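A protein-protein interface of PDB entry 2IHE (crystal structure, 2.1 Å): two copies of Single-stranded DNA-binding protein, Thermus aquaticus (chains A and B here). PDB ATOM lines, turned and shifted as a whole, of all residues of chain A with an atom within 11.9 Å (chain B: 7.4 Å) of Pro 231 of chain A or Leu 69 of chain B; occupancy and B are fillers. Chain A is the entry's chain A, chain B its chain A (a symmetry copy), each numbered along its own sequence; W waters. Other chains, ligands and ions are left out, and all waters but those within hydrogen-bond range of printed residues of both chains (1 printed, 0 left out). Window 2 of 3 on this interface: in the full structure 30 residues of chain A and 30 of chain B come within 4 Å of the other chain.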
ATOM      1  N   ALA A   2     -21.851  -9.430  10.134  1.00  0.00           N
ATOM      2  CA  ALA A   2     -22.042 -10.717  10.842  1.00  0.00           C
ATOM      3  C   ALA A   2     -20.999 -10.797  11.935  1.00  0.00           C
ATOM      4  O   ALA A   2     -20.163  -9.906  12.057  1.00  0.00           O
ATOM      5  CB  ALA A   2     -21.872 -11.876   9.869  1.00  0.00           C
ATOM      6  N   ARG A   3     -21.057 -11.857  12.740  1.00  0.00           N
ATOM      7  CA  ARG A   3     -20.079 -12.075  13.811  1.00  0.00           C
ATOM      8  C   ARG A   3     -19.133 -13.141  13.246  1.00  0.00           C
ATOM      9  O   ARG A   3     -17.949 -12.885  13.007  1.00  0.00           O
ATOM     10  CB  ARG A   3     -20.765 -12.612  15.074  1.00  0.00           C
ATOM     11  CG  ARG A   3     -20.053 -12.301  16.400  1.00  0.00           C
ATOM     12  CD  ARG A   3     -18.527 -12.438  16.328  1.00  0.00           C
ATOM     13  NE  ARG A   3     -17.881 -11.192  15.911  1.00  0.00           N
ATOM     14  CZ  ARG A   3     -16.564 -11.029  15.799  1.00  0.00           C
ATOM     15  NH1 ARG A   3     -15.748 -12.041  16.069  1.00  0.00           N
ATOM     16  NH2 ARG A   3     -16.061  -9.852  15.437  1.00  0.00           N
ATOM     17  N   PRO A 227     -12.646  -5.441  13.375  1.00  0.00           N
ATOM     18  CA  PRO A 227     -13.972  -4.854  13.561  1.00  0.00           C
ATOM     19  C   PRO A 227     -14.145  -4.420  15.002  1.00  0.00           C
ATOM     20  O   PRO A 227     -13.907  -5.204  15.913  1.00  0.00           O
ATOM     21  CB  PRO A 227     -14.906  -5.997  13.171  1.00  0.00           C
ATOM     22  CG  PRO A 227     -14.171  -7.192  13.658  1.00  0.00           C
ATOM     23  CD  PRO A 227     -12.746  -6.904  13.208  1.00  0.00           C
ATOM     24  N   THR A 228     -14.524  -3.160  15.200  1.00  0.00           N
ATOM     25  CA  THR A 228     -14.748  -2.662  16.539  1.00  0.00           C
ATOM     26  C   THR A 228     -15.956  -3.445  17.035  1.00  0.00           C
ATOM     27  O   THR A 228     -16.908  -3.660  16.279  1.00  0.00           O
ATOM     28  CB  THR A 228     -15.046  -1.164  16.527  1.00  0.00           C
ATOM     29  OG1 THR A 228     -16.077  -0.870  15.579  1.00  0.00           O
ATOM     30  CG2 THR A 228     -13.821  -0.410  16.133  1.00  0.00           C
ATOM     31  N   ARG A 229     -15.924  -3.879  18.291  1.00  0.00           N
ATOM     32  CA  ARG A 229     -17.023  -4.674  18.828  1.00  0.00           C
ATOM     33  C   ARG A 229     -18.385  -4.000  18.767  1.00  0.00           C
ATOM     34  O   ARG A 229     -18.513  -2.809  18.480  1.00  0.00           O
ATOM     35  CB  ARG A 229     -16.768  -5.054  20.282  1.00  0.00           C
ATOM     36  CG  ARG A 229     -15.323  -5.386  20.608  1.00  0.00           C
ATOM     37  CD  ARG A 229     -14.745  -6.440  19.665  1.00  0.00           C
ATOM     38  NE  ARG A 229     -13.298  -6.554  19.820  1.00  0.00           N
ATOM     39  CZ  ARG A 229     -12.466  -6.839  18.823  1.00  0.00           C
ATOM     40  NH1 ARG A 229     -12.943  -7.040  17.603  1.00  0.00           N
ATOM     41  NH2 ARG A 229     -11.160  -6.898  19.037  1.00  0.00           N
ATOM     42  N   GLY A 230     -19.463  -4.786  18.915  1.00  0.00           N
ATOM     43  CA  GLY A 230     -20.803  -4.231  18.782  1.00  0.00           C
ATOM     44  C   GLY A 230     -21.069  -3.173  19.843  1.00  0.00           C
ATOM     45  O   GLY A 230     -20.211  -2.951  20.697  1.00  0.00           O
ATOM     46  N   PRO A 231     -22.244  -2.562  19.768  1.00  0.00           N
ATOM     47  CA  PRO A 231     -22.682  -1.503  20.679  1.00  0.00           C
ATOM     48  C   PRO A 231     -22.266  -1.715  22.132  1.00  0.00           C
ATOM     49  O   PRO A 231     -22.120  -2.846  22.595  1.00  0.00           O
ATOM     50  CB  PRO A 231     -24.208  -1.597  20.549  1.00  0.00           C
ATOM     51  CG  PRO A 231     -24.401  -1.948  19.106  1.00  0.00           C
ATOM     52  CD  PRO A 231     -23.271  -2.875  18.753  1.00  0.00           C
ATOM     53  N   ALA A 232     -22.069  -0.612  22.843  1.00  0.00           N
ATOM     54  CA  ALA A 232     -21.528  -0.572  24.191  1.00  0.00           C
ATOM     55  C   ALA A 232     -22.585  -0.503  25.285  1.00  0.00           C
ATOM     56  O   ALA A 232     -23.244   0.519  25.490  1.00  0.00           O
ATOM     57  CB  ALA A 232     -20.587   0.631  24.307  1.00  0.00           C
ATOM     58  N   GLN A 233     -22.754  -1.588  26.030  1.00  0.00           N
ATOM     59  CA  GLN A 233     -23.680  -1.725  27.143  1.00  0.00           C
ATOM     60  C   GLN A 233     -23.749  -0.501  28.046  1.00  0.00           C
ATOM     61  O   GLN A 233     -23.197   0.569  27.780  1.00  0.00           O
ATOM     62  CB  GLN A 233     -23.245  -2.956  27.946  1.00  0.00           C
ATOM     63  CG  GLN A 233     -24.315  -3.603  28.807  1.00  0.00           C
ATOM     64  CD  GLN A 233     -23.889  -3.711  30.260  1.00  0.00           C
ATOM     65  OE1 GLN A 233     -23.232  -2.814  30.787  1.00  0.00           O
ATOM     66  NE2 GLN A 233     -24.259  -4.816  30.903  1.00  0.00           N
ATOM     67  N   ALA A 234     -24.449  -0.636  29.173  1.00  0.00           N
ATOM     68  CA  ALA A 234     -24.639   0.419  30.157  1.00  0.00           C
ATOM     69  C   ALA A 234     -23.360   0.720  30.932  1.00  0.00           C
ATOM     70  O   ALA A 234     -22.942   1.877  31.031  1.00  0.00           O
ATOM     71  CB  ALA A 234     -25.748   0.039  31.132  1.00  0.00           C
ATOM     72  N   GLY A 235     -22.750  -0.323  31.485  1.00  0.00           N
ATOM     73  CA  GLY A 235     -21.484  -0.261  32.181  1.00  0.00           C
ATOM     74  C   GLY A 235     -21.532   0.095  33.646  1.00  0.00           C
ATOM     75  O   GLY A 235     -22.083   1.123  34.046  1.00  0.00           O
ATOM     76  N   ARG A 238     -18.722   2.522  33.728  1.00  0.00           N
ATOM     77  CA  ARG A 238     -18.836   3.342  32.528  1.00  0.00           C
ATOM     78  C   ARG A 238     -18.585   3.075  31.047  1.00  0.00           C
ATOM     79  O   ARG A 238     -19.279   3.611  30.183  1.00  0.00           O
ATOM     80  CB  ARG A 238     -17.894   4.544  32.609  1.00  0.00           C
ATOM     81  CG  ARG A 238     -18.492   5.838  32.079  1.00  0.00           C
ATOM     82  CD  ARG A 238     -18.017   6.216  30.686  1.00  0.00           C
ATOM     83  NE  ARG A 238     -18.572   5.338  29.661  1.00  0.00           N
ATOM     84  CZ  ARG A 238     -18.712   5.673  28.385  1.00  0.00           C
ATOM     85  NH1 ARG A 238     -18.335   6.876  27.970  1.00  0.00           N
ATOM     86  NH2 ARG A 238     -19.227   4.809  27.523  1.00  0.00           N
ATOM     87  N   PRO A 239     -17.588   2.244  30.763  1.00  0.00           N
ATOM     88  CA  PRO A 239     -16.960   2.220  29.437  1.00  0.00           C
ATOM     89  C   PRO A 239     -18.061   1.389  28.787  1.00  0.00           C
ATOM     90  O   PRO A 239     -18.907   1.956  28.096  1.00  0.00           O
ATOM     91  CB  PRO A 239     -15.691   1.380  29.597  1.00  0.00           C
ATOM     92  CG  PRO A 239     -15.063   1.892  30.843  1.00  0.00           C
ATOM     93  CD  PRO A 239     -16.199   2.264  31.753  1.00  0.00           C
ATOM     94  N   LEU B  14     -18.227   6.020   5.592  1.00  0.00           N
ATOM     95  CA  LEU B  14     -19.504   6.727   5.650  1.00  0.00           C
ATOM     96  C   LEU B  14     -19.267   8.164   5.273  1.00  0.00           C
ATOM     97  O   LEU B  14     -18.363   8.801   5.797  1.00  0.00           O
ATOM     98  CB  LEU B  14     -20.101   6.665   7.052  1.00  0.00           C
ATOM     99  CG  LEU B  14     -20.885   5.401   7.371  1.00  0.00           C
ATOM    100  CD1 LEU B  14     -21.334   5.423   8.820  1.00  0.00           C
ATOM    101  CD2 LEU B  14     -22.083   5.323   6.439  1.00  0.00           C
ATOM    102  N   ARG B  17     -23.634  11.148   8.469  1.00  0.00           N
ATOM    103  CA  ARG B  17     -24.082  10.410   9.646  1.00  0.00           C
ATOM    104  C   ARG B  17     -25.384   9.702   9.261  1.00  0.00           C
ATOM    105  O   ARG B  17     -26.317  10.340   8.769  1.00  0.00           O
ATOM    106  CB  ARG B  17     -24.319  11.380  10.804  1.00  0.00           C
ATOM    107  CG  ARG B  17     -24.283  10.746  12.183  1.00  0.00           C
ATOM    108  CD  ARG B  17     -24.226  11.822  13.267  1.00  0.00           C
ATOM    109  NE  ARG B  17     -24.087  11.277  14.618  1.00  0.00           N
ATOM    110  CZ  ARG B  17     -25.055  10.653  15.288  1.00  0.00           C
ATOM    111  NH1 ARG B  17     -26.252  10.484  14.738  1.00  0.00           N
ATOM    112  NH2 ARG B  17     -24.824  10.195  16.511  1.00  0.00           N
ATOM    113  N   PRO B  18     -25.453   8.368   9.451  1.00  0.00           N
ATOM    114  CA  PRO B  18     -26.654   7.592   9.115  1.00  0.00           C
ATOM    115  C   PRO B  18     -27.888   8.130   9.836  1.00  0.00           C
ATOM    116  O   PRO B  18     -27.811   8.499  11.014  1.00  0.00           O
ATOM    117  CB  PRO B  18     -26.290   6.189   9.578  1.00  0.00           C
ATOM    118  CG  PRO B  18     -24.821   6.144   9.364  1.00  0.00           C
ATOM    119  CD  PRO B  18     -24.376   7.476   9.910  1.00  0.00           C
ATOM    120  N   LEU B  30     -32.387   1.707   7.893  1.00  0.00           N
ATOM    121  CA  LEU B  30     -31.189   2.534   8.000  1.00  0.00           C
ATOM    122  C   LEU B  30     -30.410   2.545   6.685  1.00  0.00           C
ATOM    123  O   LEU B  30     -29.969   1.500   6.213  1.00  0.00           O
ATOM    124  CB  LEU B  30     -30.296   2.008   9.130  1.00  0.00           C
ATOM    125  CG  LEU B  30     -29.099   2.860   9.550  1.00  0.00           C
ATOM    126  CD1 LEU B  30     -29.574   4.121  10.262  1.00  0.00           C
ATOM    127  CD2 LEU B  30     -28.211   2.041  10.464  1.00  0.00           C
ATOM    128  N   GLU B  64     -31.717  -1.409  13.921  1.00  0.00           N
ATOM    129  CA  GLU B  64     -32.014  -0.968  15.277  1.00  0.00           C
ATOM    130  C   GLU B  64     -30.793  -0.874  16.189  1.00  0.00           C
ATOM    131  O   GLU B  64     -30.730   0.006  17.042  1.00  0.00           O
ATOM    132  CB  GLU B  64     -33.051  -1.903  15.908  1.00  0.00           C
ATOM    133  CG  GLU B  64     -33.625  -1.418  17.235  1.00  0.00           C
ATOM    134  CD  GLU B  64     -35.004  -0.780  17.091  1.00  0.00           C
ATOM    135  OE1 GLU B  64     -35.929  -1.458  16.593  1.00  0.00           O
ATOM    136  OE2 GLU B  64     -35.160   0.396  17.480  1.00  0.00           O
ATOM    137  N   MET B  65     -29.821  -1.764  16.011  1.00  0.00           N
ATOM    138  CA  MET B  65     -28.635  -1.754  16.861  1.00  0.00           C
ATOM    139  C   MET B  65     -27.511  -0.796  16.440  1.00  0.00           C
ATOM    140  O   MET B  65     -26.565  -0.577  17.197  1.00  0.00           O
ATOM    141  CB  MET B  65     -28.075  -3.182  16.998  1.00  0.00           C
ATOM    142  CG  MET B  65     -27.659  -3.844  15.686  1.00  0.00           C
ATOM    143  SD  MET B  65     -26.549  -5.282  15.877  1.00  0.00           S
ATOM    144  CE  MET B  65     -27.708  -6.664  15.821  1.00  0.00           C
ATOM    145  N   TRP B  66     -27.610  -0.213  15.250  1.00  0.00           N
ATOM    146  CA  TRP B  66     -26.566   0.690  14.769  1.00  0.00           C
ATOM    147  C   TRP B  66     -27.021   2.123  14.480  1.00  0.00           C
ATOM    148  O   TRP B  66     -26.262   3.064  14.691  1.00  0.00           O
ATOM    149  CB  TRP B  66     -25.928   0.141  13.482  1.00  0.00           C
ATOM    150  CG  TRP B  66     -25.194  -1.158  13.611  1.00  0.00           C
ATOM    151  CD1 TRP B  66     -25.578  -2.377  13.115  1.00  0.00           C
ATOM    152  CD2 TRP B  66     -23.948  -1.370  14.269  1.00  0.00           C
ATOM    153  NE1 TRP B  66     -24.645  -3.335  13.425  1.00  0.00           N
ATOM    154  CE2 TRP B  66     -23.633  -2.744  14.135  1.00  0.00           C
ATOM    155  CE3 TRP B  66     -23.064  -0.537  14.958  1.00  0.00           C
ATOM    156  CZ2 TRP B  66     -22.468  -3.300  14.666  1.00  0.00           C
ATOM    157  CZ3 TRP B  66     -21.909  -1.088  15.486  1.00  0.00           C
ATOM    158  CH2 TRP B  66     -21.620  -2.459  15.338  1.00  0.00           C
ATOM    159  N   GLY B  67     -28.245   2.271  13.973  1.00  0.00           N
ATOM    160  CA  GLY B  67     -28.791   3.575  13.601  1.00  0.00           C
ATOM    161  C   GLY B  67     -28.771   4.671  14.645  1.00  0.00           C
ATOM    162  O   GLY B  67     -29.811   5.252  14.971  1.00  0.00           O
ATOM    163  N   ASP B  68     -27.585   4.958  15.174  1.00  0.00           N
ATOM    164  CA  ASP B  68     -27.446   5.853  16.320  1.00  0.00           C
ATOM    165  C   ASP B  68     -25.964   6.007  16.655  1.00  0.00           C
ATOM    166  O   ASP B  68     -25.544   7.025  17.205  1.00  0.00           O
ATOM    167  CB  ASP B  68     -28.404   5.442  17.440  1.00  0.00           C
ATOM    168  CG  ASP B  68     -28.337   3.959  17.749  1.00  0.00           C
ATOM    169  OD1 ASP B  68     -27.324   3.517  18.332  1.00  0.00           O
ATOM    170  OD2 ASP B  68     -29.248   3.159  17.446  1.00  0.00           O
ATOM    171  N   LEU B  69     -25.184   4.987  16.320  1.00  0.00           N
ATOM    172  CA  LEU B  69     -23.740   4.985  16.565  1.00  0.00           C
ATOM    173  C   LEU B  69     -22.758   5.275  15.450  1.00  0.00           C
ATOM    174  O   LEU B  69     -21.561   5.412  15.698  1.00  0.00           O
ATOM    175  CB  LEU B  69     -23.424   3.584  17.085  1.00  0.00           C
ATOM    176  CG  LEU B  69     -24.429   3.044  18.088  1.00  0.00           C
ATOM    177  CD1 LEU B  69     -23.956   1.728  18.683  1.00  0.00           C
ATOM    178  CD2 LEU B  69     -24.610   4.089  19.147  1.00  0.00           C
ATOM    179  N   LEU B  70     -23.255   5.353  14.224  1.00  0.00           N
ATOM    180  CA  LEU B  70     -22.376   5.583  13.093  1.00  0.00           C
ATOM    181  C   LEU B  70     -22.111   7.048  12.794  1.00  0.00           C
ATOM    182  O   LEU B  70     -23.024   7.833  12.558  1.00  0.00           O
ATOM    183  CB  LEU B  70     -22.933   4.856  11.867  1.00  0.00           C
ATOM    184  CG  LEU B  70     -23.210   3.381  12.192  1.00  0.00           C
ATOM    185  CD1 LEU B  70     -23.887   2.718  11.019  1.00  0.00           C
ATOM    186  CD2 LEU B  70     -21.912   2.662  12.549  1.00  0.00           C
ATOM    187  N   GLU B  71     -20.835   7.402  12.820  1.00  0.00           N
ATOM    188  CA  GLU B  71     -20.411   8.762  12.547  1.00  0.00           C
ATOM    189  C   GLU B  71     -19.881   8.881  11.119  1.00  0.00           C
ATOM    190  O   GLU B  71     -19.267   7.947  10.585  1.00  0.00           O
ATOM    191  CB  GLU B  71     -19.300   9.179  13.522  1.00  0.00           C
ATOM    192  CG  GLU B  71     -19.633   9.018  14.996  1.00  0.00           C
ATOM    193  CD  GLU B  71     -20.392  10.198  15.564  1.00  0.00           C
ATOM    194  OE1 GLU B  71     -21.463  10.551  15.013  1.00  0.00           O
ATOM    195  OE2 GLU B  71     -19.916  10.771  16.573  1.00  0.00           O
ATOM    196  N   LYS B  72     -20.135  10.035  10.513  1.00  0.00           N
ATOM    197  CA  LYS B  72     -19.660  10.348   9.176  1.00  0.00           C
ATOM    198  C   LYS B  72     -18.140  10.140   9.206  1.00  0.00           C
ATOM    199  O   LYS B  72     -17.460  10.688  10.066  1.00  0.00           O
ATOM    200  CB  LYS B  72     -20.000  11.810   8.879  1.00  0.00           C
ATOM    201  CG  LYS B  72     -19.490  12.371   7.568  1.00  0.00           C
ATOM    202  CD  LYS B  72     -20.022  13.792   7.375  1.00  0.00           C
ATOM    203  CE  LYS B  72     -19.706  14.351   5.988  1.00  0.00           C
ATOM    204  NZ  LYS B  72     -20.387  15.659   5.736  1.00  0.00           N
ATOM    205  N   GLN B  74     -16.729   6.978   9.314  1.00  0.00           N
ATOM    206  CA  GLN B  74     -16.464   5.633   9.797  1.00  0.00           C
ATOM    207  C   GLN B  74     -16.312   4.638   8.651  1.00  0.00           C
ATOM    208  O   GLN B  74     -17.060   4.665   7.671  1.00  0.00           O
ATOM    209  CB  GLN B  74     -17.587   5.156  10.718  1.00  0.00           C
ATOM    210  CG  GLN B  74     -17.763   6.001  11.954  1.00  0.00           C
ATOM    211  CD  GLN B  74     -18.288   5.207  13.131  1.00  0.00           C
ATOM    212  OE1 GLN B  74     -18.742   5.781  14.127  1.00  0.00           O
ATOM    213  NE2 GLN B  74     -18.215   3.877  13.033  1.00  0.00           N
ATOM    214  N   PRO B 106     -18.667  -2.043  11.685  1.00  0.00           N
ATOM    215  CA  PRO B 106     -17.796  -0.869  11.632  1.00  0.00           C
ATOM    216  C   PRO B 106     -16.365  -1.365  11.900  1.00  0.00           C
ATOM    217  O   PRO B 106     -16.165  -2.247  12.736  1.00  0.00           O
ATOM    218  CB  PRO B 106     -18.347   0.003  12.759  1.00  0.00           C
ATOM    219  CG  PRO B 106     -19.815  -0.335  12.747  1.00  0.00           C
ATOM    220  CD  PRO B 106     -19.795  -1.833  12.611  1.00  0.00           C
HETATM  221  O   HOH W   1     -18.111  -4.196  14.171  1.00  0.00           O
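O of Pro 106 of chain B sits at hydrogen-bond distance from N of Thr 228 of chain A, 3.1 Å away.
The guanidinium group (NH1) of Arg 229 of chain A lies within hydrogen-bond range of the backbone carbonyl oxygen (O) of Pro 227 of chain A (2.7 Å). The side-chain sulfur of Met 65 of chain B sits at hydrogen-bond distance from the indole nitrogen of Trp 66 of chain B (3.7 Å). The backbone carbonyl oxygen (O) of Leu 69 of chain B sits close to the side-chain amide oxygen (OE1) of Gln 74 of chain B (3.2 Å).
Among the printed residues, pairs that only touch across the chains: Pro 227 of chain A with Pro 106 of chain B (3.5 Å), Gly 230 of chain A with Trp 66 of chain B (3.96 Å), Pro 231 of chain A with Met 65 of chain B (3.2 Å), Pro 231 of chain A with Trp 66 of chain B (3.8 Å) and Pro 231 of chain A with Leu 69 of chain B (3.7 Å).
Of the printed residues of chain B, Pro 231 of chain A touches Met 65 (3.2 Å), Trp 66 (3.8 Å) and Leu 69 (3.7 Å). Printed residues of chain A within 4 Å of Leu 69 of chain B: Pro 231 (3.7 Å). No residue of chain A comes within 4 Å of Pro 18 of chain B. No residue of chain A comes within 4 Å of Glu 71 of chain B. Printed residues of chain B within 4 Å of Gly 230 of chain A: Trp 66. Of the printed residues of chain B, Thr 228 of chain A touches Pro 106 (3.1 Å). The nearest printed residue of chain B that does not touch Pro 231 of chain A is Asp 68 of chain B (6.2 Å). The nearest printed residue of chain B that does not touch Pro 227 of chain A is Trp 66 of chain B (7.7 Å).
Of the 15 printed residues of chain B, 4 touch a printed residue of chain A. Among the printed residues, no Asp or Glu carboxylate lies within 4 Å of a Lys or Arg side-chain nitrogen of the other chain.
No position is printed for both chains. Of the 6 pairs that touch across the chains among the printed residues, none has its exchanged pair printed and touching as well.
Water W1 bridges the backbone carbonyl oxygen (O) of Thr 228 of chain A (2.5 Å) and the backbone carbonyl oxygen (O) of Pro 106 of chain B (3.1 Å).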
